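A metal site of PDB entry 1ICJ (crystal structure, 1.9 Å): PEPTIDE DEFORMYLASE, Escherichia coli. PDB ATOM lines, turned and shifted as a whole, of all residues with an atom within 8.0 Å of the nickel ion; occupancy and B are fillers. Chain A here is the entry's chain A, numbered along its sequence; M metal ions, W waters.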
ATOM      1  N   VAL A   5       5.943  28.822 -31.169  1.00  0.00           N
ATOM      2  CA  VAL A   5       7.390  28.967 -31.005  1.00  0.00           C
ATOM      3  C   VAL A   5       7.970  29.677 -32.231  1.00  0.00           C
ATOM      4  O   VAL A   5       7.680  29.287 -33.366  1.00  0.00           O
ATOM      5  CB  VAL A   5       8.054  27.568 -30.839  1.00  0.00           C
ATOM      6  CG1 VAL A   5       9.573  27.704 -30.724  1.00  0.00           C
ATOM      7  CG2 VAL A   5       7.474  26.875 -29.628  1.00  0.00           C
ATOM      8  N   GLY A  45      13.919  21.737 -23.394  1.00  0.00           N
ATOM      9  CA  GLY A  45      14.097  23.036 -22.796  1.00  0.00           C
ATOM     10  C   GLY A  45      13.392  24.079 -23.637  1.00  0.00           C
ATOM     11  O   GLY A  45      13.201  23.888 -24.850  1.00  0.00           O
ATOM     12  N   LEU A  46      12.949  25.142 -22.981  1.00  0.00           N
ATOM     13  CA  LEU A  46      12.330  26.262 -23.677  1.00  0.00           C
ATOM     14  C   LEU A  46      12.591  27.554 -22.900  1.00  0.00           C
ATOM     15  O   LEU A  46      12.555  27.556 -21.667  1.00  0.00           O
ATOM     16  CB  LEU A  46      10.814  26.008 -23.822  1.00  0.00           C
ATOM     17  CG  LEU A  46       9.997  26.989 -24.675  1.00  0.00           C
ATOM     18  CD1 LEU A  46      10.365  26.843 -26.133  1.00  0.00           C
ATOM     19  CD2 LEU A  46       8.535  26.716 -24.470  1.00  0.00           C
ATOM     20  N   ALA A  47      13.009  28.601 -23.594  1.00  0.00           N
ATOM     21  CA  ALA A  47      13.185  29.904 -22.972  1.00  0.00           C
ATOM     22  C   ALA A  47      11.984  30.764 -23.360  1.00  0.00           C
ATOM     23  O   ALA A  47      11.420  30.607 -24.460  1.00  0.00           O
ATOM     24  CB  ALA A  47      14.474  30.554 -23.453  1.00  0.00           C
ATOM     25  N   GLN A  50      11.690  32.486 -26.782  1.00  0.00           N
ATOM     26  CA  GLN A  50      11.346  31.643 -27.926  1.00  0.00           C
ATOM     27  C   GLN A  50       9.856  31.718 -28.241  1.00  0.00           C
ATOM     28  O   GLN A  50       9.437  31.473 -29.361  1.00  0.00           O
ATOM     29  CB  GLN A  50      11.727  30.191 -27.674  1.00  0.00           C
ATOM     30  CG  GLN A  50      13.211  29.927 -27.767  1.00  0.00           C
ATOM     31  CD  GLN A  50      13.550  28.485 -27.498  1.00  0.00           C
ATOM     32  OE1 GLN A  50      13.845  28.119 -26.365  1.00  0.00           O
ATOM     33  NE2 GLN A  50      13.480  27.655 -28.522  1.00  0.00           N
ATOM     34  N   GLU A  88      23.540  19.784 -30.471  1.00  0.00           N
ATOM     35  CA  GLU A  88      22.354  20.422 -29.880  1.00  0.00           C
ATOM     36  C   GLU A  88      21.235  20.637 -30.896  1.00  0.00           C
ATOM     37  O   GLU A  88      21.492  20.989 -32.037  1.00  0.00           O
ATOM     38  CB  GLU A  88      22.732  21.774 -29.285  1.00  0.00           C
ATOM     39  CG  GLU A  88      23.751  21.670 -28.197  1.00  0.00           C
ATOM     40  CD  GLU A  88      24.023  22.987 -27.510  1.00  0.00           C
ATOM     41  OE1 GLU A  88      23.266  23.968 -27.688  1.00  0.00           O
ATOM     42  OE2 GLU A  88      25.024  23.054 -26.758  1.00  0.00           O
ATOM     43  N   GLY A  89      20.002  20.527 -30.417  1.00  0.00           N
ATOM     44  CA  GLY A  89      18.858  20.959 -31.207  1.00  0.00           C
ATOM     45  C   GLY A  89      18.191  22.152 -30.542  1.00  0.00           C
ATOM     46  O   GLY A  89      18.641  22.649 -29.505  1.00  0.00           O
ATOM     47  N   CYS A  90      17.115  22.631 -31.166  1.00  0.00           N
ATOM     48  CA  CYS A  90      16.403  23.813 -30.692  1.00  0.00           C
ATOM     49  C   CYS A  90      15.071  23.838 -31.426  1.00  0.00           C
ATOM     50  O   CYS A  90      15.027  23.717 -32.664  1.00  0.00           O
ATOM     51  CB  CYS A  90      17.198  25.073 -31.047  1.00  0.00           C
ATOM     52  SG  CYS A  90      16.579  26.594 -30.302  1.00  0.00           S
ATOM     53  N   LEU A  91      13.984  24.085 -30.701  1.00  0.00           N
ATOM     54  CA  LEU A  91      12.682  24.172 -31.341  1.00  0.00           C
ATOM     55  C   LEU A  91      12.542  25.382 -32.269  1.00  0.00           C
ATOM     56  O   LEU A  91      11.687  25.379 -33.152  1.00  0.00           O
ATOM     57  CB  LEU A  91      11.566  24.176 -30.286  1.00  0.00           C
ATOM     58  CG  LEU A  91      11.380  22.895 -29.470  1.00  0.00           C
ATOM     59  CD1 LEU A  91      10.373  23.173 -28.361  1.00  0.00           C
ATOM     60  CD2 LEU A  91      10.934  21.728 -30.348  1.00  0.00           C
ATOM     61  N   SER A  92      13.405  26.382 -32.100  1.00  0.00           N
ATOM     62  CA  SER A  92      13.421  27.552 -32.989  1.00  0.00           C
ATOM     63  C   SER A  92      14.258  27.342 -34.267  1.00  0.00           C
ATOM     64  O   SER A  92      14.324  28.234 -35.119  1.00  0.00           O
ATOM     65  CB  SER A  92      13.928  28.788 -32.252  1.00  0.00           C
ATOM     66  OG  SER A  92      13.024  29.178 -31.223  1.00  0.00           O
ATOM     67  N   ILE A  93      14.951  26.209 -34.340  1.00  0.00           N
ATOM     68  CA  ILE A  93      15.789  25.895 -35.492  1.00  0.00           C
ATOM     69  C   ILE A  93      15.448  24.481 -35.930  1.00  0.00           C
ATOM     70  O   ILE A  93      16.252  23.548 -35.836  1.00  0.00           O
ATOM     71  CB  ILE A  93      17.301  26.040 -35.176  1.00  0.00           C
ATOM     72  CG1 ILE A  93      17.574  27.454 -34.622  1.00  0.00           C
ATOM     73  CG2 ILE A  93      18.120  25.837 -36.440  1.00  0.00           C
ATOM     74  CD1 ILE A  93      19.001  27.733 -34.208  1.00  0.00           C
ATOM     75  N   ARG A 102      30.551  24.182 -24.993  1.00  0.00           N
ATOM     76  CA  ARG A 102      29.926  24.562 -23.737  1.00  0.00           C
ATOM     77  C   ARG A 102      30.894  24.310 -22.573  1.00  0.00           C
ATOM     78  O   ARG A 102      31.841  23.535 -22.714  1.00  0.00           O
ATOM     79  CB  ARG A 102      28.655  23.729 -23.519  1.00  0.00           C
ATOM     80  CG  ARG A 102      27.557  23.930 -24.557  1.00  0.00           C
ATOM     81  CD  ARG A 102      26.947  25.323 -24.471  1.00  0.00           C
ATOM     82  NE  ARG A 102      25.815  25.411 -25.388  1.00  0.00           N
ATOM     83  CZ  ARG A 102      25.261  26.535 -25.808  1.00  0.00           C
ATOM     84  NH1 ARG A 102      25.621  27.708 -25.308  1.00  0.00           N
ATOM     85  NH2 ARG A 102      24.284  26.477 -26.701  1.00  0.00           N
ATOM     86  N   CYS A 129      22.131  22.050 -21.382  1.00  0.00           N
ATOM     87  CA  CYS A 129      20.767  22.543 -21.558  1.00  0.00           C
ATOM     88  C   CYS A 129      20.598  23.902 -20.905  1.00  0.00           C
ATOM     89  O   CYS A 129      19.986  24.811 -21.487  1.00  0.00           O
ATOM     90  CB  CYS A 129      19.790  21.544 -20.933  1.00  0.00           C
ATOM     91  SG  CYS A 129      19.373  20.189 -21.994  1.00  0.00           S
ATOM     92  N   HIS A 132      22.461  26.528 -22.975  1.00  0.00           N
ATOM     93  CA  HIS A 132      21.710  26.752 -24.203  1.00  0.00           C
ATOM     94  C   HIS A 132      20.516  27.701 -23.934  1.00  0.00           C
ATOM     95  O   HIS A 132      20.223  28.609 -24.706  1.00  0.00           O
ATOM     96  CB  HIS A 132      21.212  25.396 -24.753  1.00  0.00           C
ATOM     97  CG  HIS A 132      20.350  25.503 -25.971  1.00  0.00           C
ATOM     98  ND1 HIS A 132      20.736  25.001 -27.202  1.00  0.00           N
ATOM     99  CD2 HIS A 132      19.103  26.009 -26.144  1.00  0.00           C
ATOM    100  CE1 HIS A 132      19.761  25.191 -28.070  1.00  0.00           C
ATOM    101  NE2 HIS A 132      18.771  25.801 -27.464  1.00  0.00           N
ATOM    102  N   GLU A 133      19.823  27.490 -22.817  1.00  0.00           N
ATOM    103  CA  GLU A 133      18.584  28.216 -22.554  1.00  0.00           C
ATOM    104  C   GLU A 133      18.905  29.609 -22.048  1.00  0.00           C
ATOM    105  O   GLU A 133      18.215  30.568 -22.393  1.00  0.00           O
ATOM    106  CB  GLU A 133      17.701  27.469 -21.548  1.00  0.00           C
ATOM    107  CG  GLU A 133      17.109  26.136 -22.070  1.00  0.00           C
ATOM    108  CD  GLU A 133      16.385  26.255 -23.403  1.00  0.00           C
ATOM    109  OE1 GLU A 133      15.841  27.344 -23.730  1.00  0.00           O
ATOM    110  OE2 GLU A 133      16.386  25.255 -24.142  1.00  0.00           O
ATOM    111  N   ASP A 135      21.455  31.323 -22.951  1.00  0.00           N
ATOM    112  CA  ASP A 135      21.805  32.048 -24.180  1.00  0.00           C
ATOM    113  C   ASP A 135      20.569  32.669 -24.840  1.00  0.00           C
ATOM    114  O   ASP A 135      20.627  33.797 -25.305  1.00  0.00           O
ATOM    115  CB  ASP A 135      22.493  31.116 -25.194  1.00  0.00           C
ATOM    116  CG  ASP A 135      24.014  31.120 -25.069  1.00  0.00           C
ATOM    117  OD1 ASP A 135      24.580  31.787 -24.175  1.00  0.00           O
ATOM    118  OD2 ASP A 135      24.622  30.403 -25.888  1.00  0.00           O
ATOM    119  N   HIS A 136      19.491  31.907 -24.955  1.00  0.00           N
ATOM    120  CA  HIS A 136      18.258  32.433 -25.554  1.00  0.00           C
ATOM    121  C   HIS A 136      17.836  33.768 -24.958  1.00  0.00           C
ATOM    122  O   HIS A 136      17.452  34.675 -25.694  1.00  0.00           O
ATOM    123  CB  HIS A 136      17.103  31.430 -25.417  1.00  0.00           C
ATOM    124  CG  HIS A 136      17.091  30.368 -26.486  1.00  0.00           C
ATOM    125  ND1 HIS A 136      16.991  30.664 -27.822  1.00  0.00           N
ATOM    126  CD2 HIS A 136      17.140  29.024 -26.390  1.00  0.00           C
ATOM    127  CE1 HIS A 136      16.977  29.537 -28.520  1.00  0.00           C
ATOM    128  NE2 HIS A 136      17.062  28.525 -27.669  1.00  0.00           N
ATOM    129  N   LYS A 140      20.978  34.918 -28.009  1.00  0.00           N
ATOM    130  CA  LYS A 140      21.913  34.036 -28.680  1.00  0.00           C
ATOM    131  C   LYS A 140      21.333  32.699 -29.080  1.00  0.00           C
ATOM    132  O   LYS A 140      20.621  32.043 -28.321  1.00  0.00           O
ATOM    133  CB  LYS A 140      23.135  33.785 -27.818  1.00  0.00           C
ATOM    134  CG  LYS A 140      23.994  34.992 -27.688  1.00  0.00           C
ATOM    135  CD  LYS A 140      25.293  34.663 -27.008  1.00  0.00           C
ATOM    136  CE  LYS A 140      26.149  33.791 -27.888  1.00  0.00           C
ATOM    137  NZ  LYS A 140      27.415  33.467 -27.169  1.00  0.00           N
ATOM    138  N   LEU A 141      21.750  32.235 -30.249  1.00  0.00           N
ATOM    139  CA  LEU A 141      21.317  30.945 -30.766  1.00  0.00           C
ATOM    140  C   LEU A 141      22.552  30.047 -30.984  1.00  0.00           C
ATOM    141  O   LEU A 141      23.660  30.560 -31.177  1.00  0.00           O
ATOM    142  CB  LEU A 141      20.585  31.158 -32.091  1.00  0.00           C
ATOM    143  CG  LEU A 141      19.357  32.067 -32.024  1.00  0.00           C
ATOM    144  CD1 LEU A 141      18.974  32.483 -33.435  1.00  0.00           C
ATOM    145  CD2 LEU A 141      18.205  31.322 -31.346  1.00  0.00           C
ATOM    146  N   PHE A 142      22.364  28.731 -31.016  1.00  0.00           N
ATOM    147  CA  PHE A 142      23.517  27.853 -31.084  1.00  0.00           C
ATOM    148  C   PHE A 142      24.273  27.996 -32.397  1.00  0.00           C
ATOM    149  O   PHE A 142      25.490  27.840 -32.434  1.00  0.00           O
ATOM    150  CB  PHE A 142      23.149  26.377 -30.779  1.00  0.00           C
ATOM    151  CG  PHE A 142      22.475  25.643 -31.920  1.00  0.00           C
ATOM    152  CD1 PHE A 142      23.176  25.290 -33.073  1.00  0.00           C
ATOM    153  CD2 PHE A 142      21.160  25.219 -31.802  1.00  0.00           C
ATOM    154  CE1 PHE A 142      22.574  24.556 -34.073  1.00  0.00           C
ATOM    155  CE2 PHE A 142      20.556  24.471 -32.804  1.00  0.00           C
ATOM    156  CZ  PHE A 142      21.260  24.129 -33.938  1.00  0.00           C
HETATM  157 NI    NI M   1      16.899  26.513 -28.063  1.00  0.00          NI
HETATM  158  O   HOH W   1      15.760  25.943 -26.524  1.00  0.00           O
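A ring nitrogen (NE2) of His 136 lies close to the side-chain amide oxygen of Gln 50 (3.5 Å). The side-chain amide oxygen of Gln 50 sits close to the side-chain carboxylate of Glu 133 (3.4 Å). The backbone NH of Ala 47 lies within hydrogen-bond range of the side-chain amide oxygen of Gln 50 (2.9 Å). The side-chain sulfur (SG) of Cys 90 lies close to the backbone NH (N) of Ser 92 (3.7 Å). The side-chain sulfur (SG) of Cys 90 lies close to the side-chain amide nitrogen (NE2) of Gln 50 (3.7 Å). The side-chain carboxylate (OE1) of Glu 88 sits at hydrogen-bond distance from a ring nitrogen (ND1) of His 132 (2.8 Å). The side-chain amide nitrogen (NE2) of Gln 50 lies within hydrogen-bond range of the side-chain hydroxyl (OG) of Ser 92 (3.1 Å).
Residues that only touch the nickel ion: Gln 50. Four residues have an atom within 4 Å of the nickel ion: Gln 50, Cys 90, His 132 and His 136.
The nickel ion is bound by water W1. NE2 of His 136 is bound to the nickel ion, at 2.1 Å. NE2 of His 132 is bound to the nickel ion (2.1 Å). The nickel ion is bound by SG of Cys 90, at 2.3 Å. The nickel ion has four donor atoms within binding distance.
Water W1 lies within hydrogen-bond range of OE2 of Glu 133 (2.6 Å) and OE1 of Gln 50 (2.9 Å).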
